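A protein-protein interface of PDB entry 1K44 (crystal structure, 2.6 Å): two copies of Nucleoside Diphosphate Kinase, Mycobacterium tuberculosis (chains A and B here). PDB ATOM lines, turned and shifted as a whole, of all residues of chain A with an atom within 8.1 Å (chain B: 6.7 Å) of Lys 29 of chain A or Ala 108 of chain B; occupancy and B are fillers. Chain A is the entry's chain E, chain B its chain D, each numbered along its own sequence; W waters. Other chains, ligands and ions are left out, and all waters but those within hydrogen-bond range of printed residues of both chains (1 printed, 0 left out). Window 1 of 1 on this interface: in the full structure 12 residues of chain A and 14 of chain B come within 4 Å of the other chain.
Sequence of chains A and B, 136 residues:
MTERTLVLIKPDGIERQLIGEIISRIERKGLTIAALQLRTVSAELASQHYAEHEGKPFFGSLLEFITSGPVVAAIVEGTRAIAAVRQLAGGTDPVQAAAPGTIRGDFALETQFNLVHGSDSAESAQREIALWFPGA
Among the printed residues, pairs that only touch across the chains: Lys 29 of chain A with Asp 106 of chain B, Thr 79 of chain A with Leu 109 of chain B, Arg 28 of chain A with Phe 107 of chain B, Arg 28 of chain A with Asp 106 of chain B, Gln 87 of chain A with Val 95 of chain B, Lys 29 of chain A with Leu 109 of chain B, Arg 80 of chain A with Val 95 of chain B, Lys 29 of chain A with Arg 104 of chain B, Leu 31 of chain A with Leu 109 of chain B, Gly 30 of chain A with Leu 109 of chain B, Thr 79 of chain A with Glu 110 of chain B, Ala 83 of chain A with Val 95 of chain B, Ala 84 of chain A with Leu 109 of chain B, Gly 30 of chain A with Arg 16 of chain B and Gln 87 of chain A with Gly 105 of chain B.
The backbone carbonyl oxygen of Asn 114 of chain B lies within hydrogen-bond range of the guanidinium group of Arg 104 of chain B (3.2 Å).
The side-chain amino group of Lys 29 of chain A lies close to the side-chain amide nitrogen of Gln 87 of chain A (2.9 Å).
The backbone carbonyl oxygen of Ile 26 of chain A is in hydrogen-bond range of the backbone NH of Leu 31 of chain A, 3.4 Å away.
O of Phe 107 of chain B lies within hydrogen-bond range of NH1 of Arg 16 of chain B.
Of the 19 printed residues of chain A, 9 touch a printed residue of chain B.
Hydrophobic or aromatic side chains of chain A within 4 Å of the printed part of chain B: Leu 31, Ala 83 and Ala 84.
Of the 18 printed residues of chain B, 11 touch a printed residue of chain A.
Printed residues of chain B that touch a printed residue of chain A: Arg 16, Pro 94, Val 95, Ala 98, Arg 104, Gly 105, Asp 106, Phe 107, Ala 108, Leu 109 and Glu 110.
Hydrophobic or aromatic side chains of chain B within 4 Å of the printed part of chain A: Val 95, Phe 107 and Leu 109.
Among the printed residues, 23 pairs touch across the chains.
The backbone carbonyl oxygen of Ala 108 of chain B is in hydrogen-bond range of the side-chain amino group of Lys 29 of chain A (2.8 Å).
The backbone carbonyl oxygen (O) of Pro 94 of chain B sits at hydrogen-bond distance from the side-chain amino group (NZ) of Lys 29 of chain A.
NH2 of Arg 16 of chain B is in hydrogen-bond range of O of Arg 28 of chain A (3.0 Å).
The guanidinium group of Arg 80 of chain A sits at hydrogen-bond distance from the backbone carbonyl oxygen of Leu 109 of chain B (3.1 Å).
O of Gly 105 of chain B lies within hydrogen-bond range of NZ of Lys 29 of chain A (2.7 Å).
O of Pro 94 of chain B lies close to OE1 of Gln 87 of chain A, at 2.8 Å.
O of Phe 107 of chain B lies close to O of Lys 29 of chain A (3.3 Å).
The backbone carbonyl oxygen of Ala 98 of chain B lies close to the side-chain amide oxygen of Gln 87 of chain A (2.9 Å).
Water W1 bridges the side-chain carboxylate of Asp 106 of chain B and the guanidinium group of Arg 28 of chain A.
No position is printed for both chains.
Lys 29 of chain A touches just these residues of chain B: Pro 94, Arg 104, Gly 105, Asp 106, Phe 107, Ala 108 and Leu 109.
Ala 108 of chain B touches one residue of chain A.
Of the printed residues of chain A, Phe 107 of chain B touches Arg 28 (3.4 Å) and Lys 29 (3.3 Å).
Printed residues of chain A within 4 Å of Pro 94 of chain B: Lys 29 and Gln 87.
Printed residues of chain A within 4 Å of Arg 16 of chain B: Arg 28 and Gly 30.
Of the printed residues of chain B, Ala 83 of chain A touches Val 95 (3.9 Å).
The nearest residue of chain A that does not touch Ala 108 of chain B is Arg 28 of chain A (5.2 Å).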
ATOM      1  N   ILE A  23     -28.818 -27.332 -30.363  1.00  0.00           N
ATOM      2  CA  ILE A  23     -28.445 -27.732 -29.016  1.00  0.00           C
ATOM      3  C   ILE A  23     -26.945 -28.014 -28.930  1.00  0.00           C
ATOM      4  O   ILE A  23     -26.292 -27.645 -27.956  1.00  0.00           O
ATOM      5  CB  ILE A  23     -29.263 -28.967 -28.560  1.00  0.00           C
ATOM      6  CG1 ILE A  23     -30.710 -28.537 -28.287  1.00  0.00           C
ATOM      7  CG2 ILE A  23     -28.638 -29.597 -27.319  1.00  0.00           C
ATOM      8  CD1 ILE A  23     -31.663 -29.683 -28.079  1.00  0.00           C
ATOM      9  N   SER A  24     -26.394 -28.667 -29.950  1.00  0.00           N
ATOM     10  CA  SER A  24     -24.962 -28.950 -29.970  1.00  0.00           C
ATOM     11  C   SER A  24     -24.148 -27.677 -29.801  1.00  0.00           C
ATOM     12  O   SER A  24     -23.189 -27.647 -29.021  1.00  0.00           O
ATOM     13  CB  SER A  24     -24.556 -29.598 -31.284  1.00  0.00           C
ATOM     14  OG  SER A  24     -24.866 -30.971 -31.271  1.00  0.00           O
ATOM     15  N   ARG A  25     -24.519 -26.630 -30.541  1.00  0.00           N
ATOM     16  CA  ARG A  25     -23.810 -25.366 -30.463  1.00  0.00           C
ATOM     17  C   ARG A  25     -23.857 -24.783 -29.055  1.00  0.00           C
ATOM     18  O   ARG A  25     -22.889 -24.169 -28.598  1.00  0.00           O
ATOM     19  CB  ARG A  25     -24.394 -24.381 -31.460  1.00  0.00           C
ATOM     20  CG  ARG A  25     -24.306 -24.891 -32.857  1.00  0.00           C
ATOM     21  CD  ARG A  25     -24.403 -23.774 -33.845  1.00  0.00           C
ATOM     22  NE  ARG A  25     -24.244 -24.260 -35.212  1.00  0.00           N
ATOM     23  CZ  ARG A  25     -23.935 -23.479 -36.238  1.00  0.00           C
ATOM     24  NH1 ARG A  25     -23.750 -22.174 -36.047  1.00  0.00           N
ATOM     25  NH2 ARG A  25     -23.814 -24.005 -37.449  1.00  0.00           N
ATOM     26  N   ILE A  26     -24.978 -24.969 -28.365  1.00  0.00           N
ATOM     27  CA  ILE A  26     -25.087 -24.475 -27.002  1.00  0.00           C
ATOM     28  C   ILE A  26     -24.189 -25.328 -26.104  1.00  0.00           C
ATOM     29  O   ILE A  26     -23.464 -24.797 -25.257  1.00  0.00           O
ATOM     30  CB  ILE A  26     -26.558 -24.533 -26.496  1.00  0.00           C
ATOM     31  CG1 ILE A  26     -27.421 -23.560 -27.311  1.00  0.00           C
ATOM     32  CG2 ILE A  26     -26.634 -24.186 -25.013  1.00  0.00           C
ATOM     33  CD1 ILE A  26     -28.904 -23.706 -27.068  1.00  0.00           C
ATOM     34  N   GLU A  27     -24.214 -26.645 -26.303  1.00  0.00           N
ATOM     35  CA  GLU A  27     -23.398 -27.542 -25.494  1.00  0.00           C
ATOM     36  C   GLU A  27     -21.894 -27.332 -25.684  1.00  0.00           C
ATOM     37  O   GLU A  27     -21.137 -27.272 -24.706  1.00  0.00           O
ATOM     38  CB  GLU A  27     -23.735 -29.007 -25.792  1.00  0.00           C
ATOM     39  CG  GLU A  27     -25.050 -29.492 -25.230  1.00  0.00           C
ATOM     40  CD  GLU A  27     -25.364 -30.906 -25.674  1.00  0.00           C
ATOM     41  OE1 GLU A  27     -25.555 -31.121 -26.894  1.00  0.00           O
ATOM     42  OE2 GLU A  27     -25.417 -31.806 -24.802  1.00  0.00           O
ATOM     43  N   ARG A  28     -21.455 -27.214 -26.929  1.00  0.00           N
ATOM     44  CA  ARG A  28     -20.030 -27.052 -27.177  1.00  0.00           C
ATOM     45  C   ARG A  28     -19.524 -25.688 -26.729  1.00  0.00           C
ATOM     46  O   ARG A  28     -18.321 -25.482 -26.587  1.00  0.00           O
ATOM     47  CB  ARG A  28     -19.704 -27.289 -28.660  1.00  0.00           C
ATOM     48  CG  ARG A  28     -20.243 -26.227 -29.595  1.00  0.00           C
ATOM     49  CD  ARG A  28     -19.735 -26.405 -31.030  1.00  0.00           C
ATOM     50  NE  ARG A  28     -20.218 -25.344 -31.916  1.00  0.00           N
ATOM     51  CZ  ARG A  28     -19.852 -25.202 -33.188  1.00  0.00           C
ATOM     52  NH1 ARG A  28     -18.989 -26.058 -33.729  1.00  0.00           N
ATOM     53  NH2 ARG A  28     -20.352 -24.208 -33.926  1.00  0.00           N
ATOM     54  N   LYS A  29     -20.444 -24.754 -26.506  1.00  0.00           N
ATOM     55  CA  LYS A  29     -20.076 -23.420 -26.053  1.00  0.00           C
ATOM     56  C   LYS A  29     -19.735 -23.482 -24.561  1.00  0.00           C
ATOM     57  O   LYS A  29     -19.143 -22.552 -24.009  1.00  0.00           O
ATOM     58  CB  LYS A  29     -21.228 -22.447 -26.287  1.00  0.00           C
ATOM     59  CG  LYS A  29     -20.987 -21.023 -25.771  1.00  0.00           C
ATOM     60  CD  LYS A  29     -19.923 -20.284 -26.560  1.00  0.00           C
ATOM     61  CE  LYS A  29     -19.925 -18.810 -26.215  1.00  0.00           C
ATOM     62  NZ  LYS A  29     -18.857 -18.040 -26.909  1.00  0.00           N
ATOM     63  N   GLY A  30     -20.113 -24.583 -23.916  1.00  0.00           N
ATOM     64  CA  GLY A  30     -19.815 -24.746 -22.507  1.00  0.00           C
ATOM     65  C   GLY A  30     -20.996 -24.516 -21.594  1.00  0.00           C
ATOM     66  O   GLY A  30     -20.855 -24.588 -20.370  1.00  0.00           O
ATOM     67  N   LEU A  31     -22.161 -24.240 -22.180  1.00  0.00           N
ATOM     68  CA  LEU A  31     -23.375 -24.003 -21.401  1.00  0.00           C
ATOM     69  C   LEU A  31     -24.100 -25.326 -21.108  1.00  0.00           C
ATOM     70  O   LEU A  31     -23.873 -26.332 -21.790  1.00  0.00           O
ATOM     71  CB  LEU A  31     -24.297 -23.059 -22.170  1.00  0.00           C
ATOM     72  CG  LEU A  31     -23.677 -21.695 -22.453  1.00  0.00           C
ATOM     73  CD1 LEU A  31     -24.477 -20.954 -23.518  1.00  0.00           C
ATOM     74  CD2 LEU A  31     -23.615 -20.915 -21.153  1.00  0.00           C
ATOM     75  N   THR A  32     -24.963 -25.337 -20.096  1.00  0.00           N
ATOM     76  CA  THR A  32     -25.674 -26.564 -19.773  1.00  0.00           C
ATOM     77  C   THR A  32     -27.188 -26.419 -19.949  1.00  0.00           C
ATOM     78  O   THR A  32     -27.753 -25.349 -19.736  1.00  0.00           O
ATOM     79  CB  THR A  32     -25.355 -27.044 -18.322  1.00  0.00           C
ATOM     80  OG1 THR A  32     -26.003 -26.199 -17.374  1.00  0.00           O
ATOM     81  CG2 THR A  32     -23.867 -26.983 -18.053  1.00  0.00           C
ATOM     82  N   VAL A  76     -31.323 -22.550 -20.558  1.00  0.00           N
ATOM     83  CA  VAL A  76     -29.881 -22.682 -20.692  1.00  0.00           C
ATOM     84  C   VAL A  76     -29.252 -21.969 -19.504  1.00  0.00           C
ATOM     85  O   VAL A  76     -29.606 -20.832 -19.187  1.00  0.00           O
ATOM     86  CB  VAL A  76     -29.386 -22.084 -22.032  1.00  0.00           C
ATOM     87  CG1 VAL A  76     -27.864 -22.102 -22.094  1.00  0.00           C
ATOM     88  CG2 VAL A  76     -29.963 -22.888 -23.180  1.00  0.00           C
ATOM     89  N   THR A  79     -22.244 -19.473 -17.055  1.00  0.00           N
ATOM     90  CA  THR A  79     -21.605 -18.162 -17.020  1.00  0.00           C
ATOM     91  C   THR A  79     -21.938 -17.333 -18.262  1.00  0.00           C
ATOM     92  O   THR A  79     -21.754 -17.802 -19.382  1.00  0.00           O
ATOM     93  CB  THR A  79     -20.075 -18.312 -16.943  1.00  0.00           C
ATOM     94  OG1 THR A  79     -19.737 -19.121 -15.812  1.00  0.00           O
ATOM     95  CG2 THR A  79     -19.407 -16.950 -16.810  1.00  0.00           C
ATOM     96  N   ARG A  80     -22.419 -16.109 -18.058  1.00  0.00           N
ATOM     97  CA  ARG A  80     -22.761 -15.211 -19.163  1.00  0.00           C
ATOM     98  C   ARG A  80     -23.746 -15.826 -20.158  1.00  0.00           C
ATOM     99  O   ARG A  80     -23.779 -15.451 -21.331  1.00  0.00           O
ATOM    100  CB  ARG A  80     -21.485 -14.786 -19.911  1.00  0.00           C
ATOM    101  CG  ARG A  80     -20.939 -13.415 -19.517  1.00  0.00           C
ATOM    102  CD  ARG A  80     -19.574 -13.516 -18.861  1.00  0.00           C
ATOM    103  NE  ARG A  80     -18.473 -13.722 -19.806  1.00  0.00           N
ATOM    104  CZ  ARG A  80     -18.019 -12.808 -20.664  1.00  0.00           C
ATOM    105  NH1 ARG A  80     -18.565 -11.597 -20.722  1.00  0.00           N
ATOM    106  NH2 ARG A  80     -16.992 -13.103 -21.452  1.00  0.00           N
ATOM    107  N   ALA A  81     -24.556 -16.760 -19.674  1.00  0.00           N
ATOM    108  CA  ALA A  81     -25.527 -17.464 -20.505  1.00  0.00           C
ATOM    109  C   ALA A  81     -26.412 -16.588 -21.397  1.00  0.00           C
ATOM    110  O   ALA A  81     -26.615 -16.891 -22.580  1.00  0.00           O
ATOM    111  CB  ALA A  81     -26.401 -18.352 -19.622  1.00  0.00           C
ATOM    112  N   ALA A  83     -25.953 -13.475 -22.613  1.00  0.00           N
ATOM    113  CA  ALA A  83     -25.197 -12.874 -23.704  1.00  0.00           C
ATOM    114  C   ALA A  83     -24.621 -13.931 -24.645  1.00  0.00           C
ATOM    115  O   ALA A  83     -24.547 -13.715 -25.862  1.00  0.00           O
ATOM    116  CB  ALA A  83     -24.080 -11.995 -23.150  1.00  0.00           C
ATOM    117  N   ALA A  84     -24.211 -15.064 -24.083  1.00  0.00           N
ATOM    118  CA  ALA A  84     -23.642 -16.150 -24.881  1.00  0.00           C
ATOM    119  C   ALA A  84     -24.651 -16.713 -25.888  1.00  0.00           C
ATOM    120  O   ALA A  84     -24.322 -16.911 -27.060  1.00  0.00           O
ATOM    121  CB  ALA A  84     -23.129 -17.269 -23.963  1.00  0.00           C
ATOM    122  N   VAL A  85     -25.874 -16.976 -25.435  1.00  0.00           N
ATOM    123  CA  VAL A  85     -26.885 -17.504 -26.329  1.00  0.00           C
ATOM    124  C   VAL A  85     -27.186 -16.499 -27.439  1.00  0.00           C
ATOM    125  O   VAL A  85     -27.410 -16.884 -28.586  1.00  0.00           O
ATOM    126  CB  VAL A  85     -28.176 -17.868 -25.560  1.00  0.00           C
ATOM    127  CG1 VAL A  85     -29.341 -18.036 -26.520  1.00  0.00           C
ATOM    128  CG2 VAL A  85     -27.960 -19.164 -24.792  1.00  0.00           C
ATOM    129  N   GLN A  87     -25.091 -14.255 -28.667  1.00  0.00           N
ATOM    130  CA  GLN A  87     -23.918 -14.293 -29.537  1.00  0.00           C
ATOM    131  C   GLN A  87     -24.058 -15.469 -30.503  1.00  0.00           C
ATOM    132  O   GLN A  87     -23.872 -15.324 -31.707  1.00  0.00           O
ATOM    133  CB  GLN A  87     -22.658 -14.489 -28.693  1.00  0.00           C
ATOM    134  CG  GLN A  87     -21.365 -14.518 -29.476  1.00  0.00           C
ATOM    135  CD  GLN A  87     -20.195 -15.049 -28.659  1.00  0.00           C
ATOM    136  OE1 GLN A  87     -19.034 -14.902 -29.052  1.00  0.00           O
ATOM    137  NE2 GLN A  87     -20.492 -15.684 -27.530  1.00  0.00           N
ATOM    138  N   LEU A  88     -24.392 -16.634 -29.951  1.00  0.00           N
ATOM    139  CA  LEU A  88     -24.572 -17.861 -30.724  1.00  0.00           C
ATOM    140  C   LEU A  88     -25.682 -17.766 -31.776  1.00  0.00           C
ATOM    141  O   LEU A  88     -25.529 -18.259 -32.901  1.00  0.00           O
ATOM    142  CB  LEU A  88     -24.892 -19.018 -29.776  1.00  0.00           C
ATOM    143  CG  LEU A  88     -23.844 -20.067 -29.409  1.00  0.00           C
ATOM    144  CD1 LEU A  88     -22.460 -19.472 -29.280  1.00  0.00           C
ATOM    145  CD2 LEU A  88     -24.281 -20.713 -28.110  1.00  0.00           C
ATOM    146  N   ASP B  12      -7.097 -25.818 -20.223  1.00  0.00           N
ATOM    147  CA  ASP B  12      -8.542 -25.900 -20.351  1.00  0.00           C
ATOM    148  C   ASP B  12      -8.906 -26.463 -21.714  1.00  0.00           C
ATOM    149  O   ASP B  12      -9.895 -27.180 -21.849  1.00  0.00           O
ATOM    150  CB  ASP B  12      -9.188 -24.525 -20.120  1.00  0.00           C
ATOM    151  CG  ASP B  12      -8.664 -23.459 -21.064  1.00  0.00           C
ATOM    152  OD1 ASP B  12      -7.437 -23.378 -21.247  1.00  0.00           O
ATOM    153  OD2 ASP B  12      -9.477 -22.694 -21.616  1.00  0.00           O
ATOM    154  N   ARG B  16     -10.937 -30.105 -22.105  1.00  0.00           N
ATOM    155  CA  ARG B  16     -12.207 -30.158 -22.808  1.00  0.00           C
ATOM    156  C   ARG B  16     -12.147 -30.953 -24.108  1.00  0.00           C
ATOM    157  O   ARG B  16     -13.110 -30.972 -24.871  1.00  0.00           O
ATOM    158  CB  ARG B  16     -12.712 -28.742 -23.059  1.00  0.00           C
ATOM    159  CG  ARG B  16     -13.063 -28.026 -21.755  1.00  0.00           C
ATOM    160  CD  ARG B  16     -13.696 -26.695 -22.019  1.00  0.00           C
ATOM    161  NE  ARG B  16     -14.885 -26.829 -22.851  1.00  0.00           N
ATOM    162  CZ  ARG B  16     -15.426 -25.820 -23.522  1.00  0.00           C
ATOM    163  NH1 ARG B  16     -14.873 -24.616 -23.449  1.00  0.00           N
ATOM    164  NH2 ARG B  16     -16.502 -26.011 -24.270  1.00  0.00           N
ATOM    165  N   LEU B  18     -10.302 -30.580 -26.992  1.00  0.00           N
ATOM    166  CA  LEU B  18     -10.418 -29.792 -28.207  1.00  0.00           C
ATOM    167  C   LEU B  18      -9.117 -29.717 -28.987  1.00  0.00           C
ATOM    168  O   LEU B  18      -8.973 -28.874 -29.868  1.00  0.00           O
ATOM    169  CB  LEU B  18     -10.897 -28.384 -27.870  1.00  0.00           C
ATOM    170  CG  LEU B  18     -12.334 -28.274 -27.337  1.00  0.00           C
ATOM    171  CD1 LEU B  18     -12.579 -26.855 -26.833  1.00  0.00           C
ATOM    172  CD2 LEU B  18     -13.333 -28.638 -28.432  1.00  0.00           C
ATOM    173  N   PRO B  94     -14.172 -14.216 -25.034  1.00  0.00           N
ATOM    174  CA  PRO B  94     -14.943 -15.144 -25.873  1.00  0.00           C
ATOM    175  C   PRO B  94     -16.409 -14.799 -26.150  1.00  0.00           C
ATOM    176  O   PRO B  94     -16.990 -15.296 -27.118  1.00  0.00           O
ATOM    177  CB  PRO B  94     -14.771 -16.486 -25.155  1.00  0.00           C
ATOM    178  CG  PRO B  94     -14.576 -16.095 -23.738  1.00  0.00           C
ATOM    179  CD  PRO B  94     -13.665 -14.899 -23.830  1.00  0.00           C
ATOM    180  N   VAL B  95     -17.010 -13.950 -25.324  1.00  0.00           N
ATOM    181  CA  VAL B  95     -18.403 -13.572 -25.540  1.00  0.00           C
ATOM    182  C   VAL B  95     -18.583 -12.176 -26.129  1.00  0.00           C
ATOM    183  O   VAL B  95     -19.452 -11.964 -26.973  1.00  0.00           O
ATOM    184  CB  VAL B  95     -19.215 -13.670 -24.232  1.00  0.00           C
ATOM    185  CG1 VAL B  95     -20.621 -13.129 -24.445  1.00  0.00           C
ATOM    186  CG2 VAL B  95     -19.283 -15.122 -23.779  1.00  0.00           C
ATOM    187  N   ALA B  98     -14.769 -12.108 -29.245  1.00  0.00           N
ATOM    188  CA  ALA B  98     -14.602 -13.158 -30.237  1.00  0.00           C
ATOM    189  C   ALA B  98     -15.879 -13.378 -31.032  1.00  0.00           C
ATOM    190  O   ALA B  98     -16.957 -13.515 -30.468  1.00  0.00           O
ATOM    191  CB  ALA B  98     -14.171 -14.446 -29.563  1.00  0.00           C
ATOM    192  N   ILE B 103     -12.403 -19.940 -32.641  1.00  0.00           N
ATOM    193  CA  ILE B 103     -12.210 -20.940 -31.601  1.00  0.00           C
ATOM    194  C   ILE B 103     -12.827 -20.493 -30.276  1.00  0.00           C
ATOM    195  O   ILE B 103     -13.578 -21.240 -29.647  1.00  0.00           O
ATOM    196  CB  ILE B 103     -10.708 -21.230 -31.406  1.00  0.00           C
ATOM    197  CG1 ILE B 103     -10.132 -21.797 -32.705  1.00  0.00           C
ATOM    198  CG2 ILE B 103     -10.496 -22.210 -30.244  1.00  0.00           C
ATOM    199  CD1 ILE B 103      -8.639 -22.085 -32.649  1.00  0.00           C
ATOM    200  N   ARG B 104     -12.525 -19.271 -29.854  1.00  0.00           N
ATOM    201  CA  ARG B 104     -13.071 -18.769 -28.601  1.00  0.00           C
ATOM    202  C   ARG B 104     -14.564 -18.507 -28.704  1.00  0.00           C
ATOM    203  O   ARG B 104     -15.314 -18.769 -27.766  1.00  0.00           O
ATOM    204  CB  ARG B 104     -12.332 -17.507 -28.188  1.00  0.00           C
ATOM    205  CG  ARG B 104     -10.911 -17.787 -27.782  1.00  0.00           C
ATOM    206  CD  ARG B 104     -10.080 -16.529 -27.736  1.00  0.00           C
ATOM    207  NE  ARG B 104      -8.745 -16.805 -27.218  1.00  0.00           N
ATOM    208  CZ  ARG B 104      -7.739 -15.942 -27.268  1.00  0.00           C
ATOM    209  NH1 ARG B 104      -7.924 -14.752 -27.819  1.00  0.00           N
ATOM    210  NH2 ARG B 104      -6.552 -16.272 -26.771  1.00  0.00           N
ATOM    211  N   GLY B 105     -14.993 -18.009 -29.861  1.00  0.00           N
ATOM    212  CA  GLY B 105     -16.400 -17.722 -30.059  1.00  0.00           C
ATOM    213  C   GLY B 105     -17.285 -18.956 -30.005  1.00  0.00           C
ATOM    214  O   GLY B 105     -18.393 -18.901 -29.463  1.00  0.00           O
ATOM    215  N   ASP B 106     -16.807 -20.073 -30.554  1.00  0.00           N
ATOM    216  CA  ASP B 106     -17.607 -21.295 -30.567  1.00  0.00           C
ATOM    217  C   ASP B 106     -17.525 -22.124 -29.288  1.00  0.00           C
ATOM    218  O   ASP B 106     -18.486 -22.790 -28.916  1.00  0.00           O
ATOM    219  CB  ASP B 106     -17.205 -22.218 -31.736  1.00  0.00           C
ATOM    220  CG  ASP B 106     -17.525 -21.630 -33.106  1.00  0.00           C
ATOM    221  OD1 ASP B 106     -18.398 -20.737 -33.190  1.00  0.00           O
ATOM    222  OD2 ASP B 106     -16.914 -22.078 -34.109  1.00  0.00           O
ATOM    223  N   PHE B 107     -16.391 -22.067 -28.601  1.00  0.00           N
ATOM    224  CA  PHE B 107     -16.196 -22.926 -27.436  1.00  0.00           C
ATOM    225  C   PHE B 107     -15.967 -22.330 -26.062  1.00  0.00           C
ATOM    226  O   PHE B 107     -16.064 -23.051 -25.079  1.00  0.00           O
ATOM    227  CB  PHE B 107     -15.017 -23.873 -27.709  1.00  0.00           C
ATOM    228  CG  PHE B 107     -15.133 -24.650 -28.991  1.00  0.00           C
ATOM    229  CD1 PHE B 107     -16.102 -25.647 -29.138  1.00  0.00           C
ATOM    230  CD2 PHE B 107     -14.260 -24.404 -30.046  1.00  0.00           C
ATOM    231  CE1 PHE B 107     -16.200 -26.399 -30.323  1.00  0.00           C
ATOM    232  CE2 PHE B 107     -14.346 -25.144 -31.236  1.00  0.00           C
ATOM    233  CZ  PHE B 107     -15.321 -26.148 -31.373  1.00  0.00           C
ATOM    234  N   ALA B 108     -15.661 -21.041 -25.976  1.00  0.00           N
ATOM    235  CA  ALA B 108     -15.359 -20.449 -24.679  1.00  0.00           C
ATOM    236  C   ALA B 108     -16.390 -19.482 -24.113  1.00  0.00           C
ATOM    237  O   ALA B 108     -17.185 -18.897 -24.846  1.00  0.00           O
ATOM    238  CB  ALA B 108     -13.986 -19.781 -24.739  1.00  0.00           C
ATOM    239  N   LEU B 109     -16.341 -19.317 -22.794  1.00  0.00           N
ATOM    240  CA  LEU B 109     -17.265 -18.463 -22.062  1.00  0.00           C
ATOM    241  C   LEU B 109     -16.562 -17.336 -21.303  1.00  0.00           C
ATOM    242  O   LEU B 109     -17.016 -16.197 -21.311  1.00  0.00           O
ATOM    243  CB  LEU B 109     -18.059 -19.325 -21.082  1.00  0.00           C
ATOM    244  CG  LEU B 109     -19.572 -19.523 -21.237  1.00  0.00           C
ATOM    245  CD1 LEU B 109     -20.051 -19.190 -22.622  1.00  0.00           C
ATOM    246  CD2 LEU B 109     -19.908 -20.958 -20.871  1.00  0.00           C
ATOM    247  N   GLU B 110     -15.444 -17.659 -20.661  1.00  0.00           N
ATOM    248  CA  GLU B 110     -14.699 -16.680 -19.874  1.00  0.00           C
ATOM    249  C   GLU B 110     -13.308 -16.393 -20.420  1.00  0.00           C
ATOM    250  O   GLU B 110     -12.691 -17.246 -21.042  1.00  0.00           O
ATOM    251  CB  GLU B 110     -14.547 -17.185 -18.440  1.00  0.00           C
ATOM    252  CG  GLU B 110     -15.801 -17.759 -17.861  1.00  0.00           C
ATOM    253  CD  GLU B 110     -15.576 -18.333 -16.487  1.00  0.00           C
ATOM    254  OE1 GLU B 110     -15.291 -17.553 -15.552  1.00  0.00           O
ATOM    255  OE2 GLU B 110     -15.680 -19.569 -16.350  1.00  0.00           O
ATOM    256  N   THR B 111     -12.809 -15.194 -20.154  1.00  0.00           N
ATOM    257  CA  THR B 111     -11.486 -14.797 -20.609  1.00  0.00           C
ATOM    258  C   THR B 111     -10.390 -15.636 -19.957  1.00  0.00           C
ATOM    259  O   THR B 111      -9.390 -15.955 -20.590  1.00  0.00           O
ATOM    260  CB  THR B 111     -11.227 -13.306 -20.304  1.00  0.00           C
ATOM    261  OG1 THR B 111     -12.204 -12.505 -20.984  1.00  0.00           O
ATOM    262  CG2 THR B 111      -9.845 -12.897 -20.772  1.00  0.00           C
ATOM    263  N   PHE B 113     -10.415 -18.733 -19.143  1.00  0.00           N
ATOM    264  CA  PHE B 113     -10.311 -20.010 -19.842  1.00  0.00           C
ATOM    265  C   PHE B 113     -10.662 -19.865 -21.310  1.00  0.00           C
ATOM    266  O   PHE B 113     -11.688 -20.376 -21.758  1.00  0.00           O
ATOM    267  CB  PHE B 113     -11.239 -21.033 -19.182  1.00  0.00           C
ATOM    268  CG  PHE B 113     -11.053 -21.129 -17.701  1.00  0.00           C
ATOM    269  CD1 PHE B 113      -9.821 -21.507 -17.171  1.00  0.00           C
ATOM    270  CD2 PHE B 113     -12.086 -20.789 -16.830  1.00  0.00           C
ATOM    271  CE1 PHE B 113      -9.616 -21.544 -15.794  1.00  0.00           C
ATOM    272  CE2 PHE B 113     -11.893 -20.823 -15.446  1.00  0.00           C
ATOM    273  CZ  PHE B 113     -10.655 -21.201 -14.927  1.00  0.00           C
ATOM    274  N   ASN B 114      -9.808 -19.175 -22.060  1.00  0.00           N
ATOM    275  CA  ASN B 114     -10.085 -18.980 -23.468  1.00  0.00           C
ATOM    276  C   ASN B 114      -9.314 -19.906 -24.413  1.00  0.00           C
ATOM    277  O   ASN B 114      -8.997 -19.545 -25.547  1.00  0.00           O
ATOM    278  CB  ASN B 114      -9.926 -17.501 -23.858  1.00  0.00           C
ATOM    279  CG  ASN B 114      -8.536 -16.981 -23.642  1.00  0.00           C
ATOM    280  OD1 ASN B 114      -7.647 -17.701 -23.187  1.00  0.00           O
ATOM    281  ND2 ASN B 114      -8.335 -15.715 -23.972  1.00  0.00           N
ATOM    282  N   LEU B 115      -8.999 -21.091 -23.899  1.00  0.00           N
ATOM    283  CA  LEU B 115      -8.389 -22.182 -24.658  1.00  0.00           C
ATOM    284  C   LEU B 115      -7.055 -22.147 -25.383  1.00  0.00           C
ATOM    285  O   LEU B 115      -6.263 -23.079 -25.269  1.00  0.00           O
ATOM    286  CB  LEU B 115      -9.417 -22.665 -25.683  1.00  0.00           C
ATOM    287  CG  LEU B 115     -10.819 -22.920 -25.139  1.00  0.00           C
ATOM    288  CD1 LEU B 115     -11.824 -22.920 -26.270  1.00  0.00           C
ATOM    289  CD2 LEU B 115     -10.834 -24.233 -24.381  1.00  0.00           C
HETATM  290  O   HOH W   1     -19.768 -21.699 -35.786  1.00  0.00           O
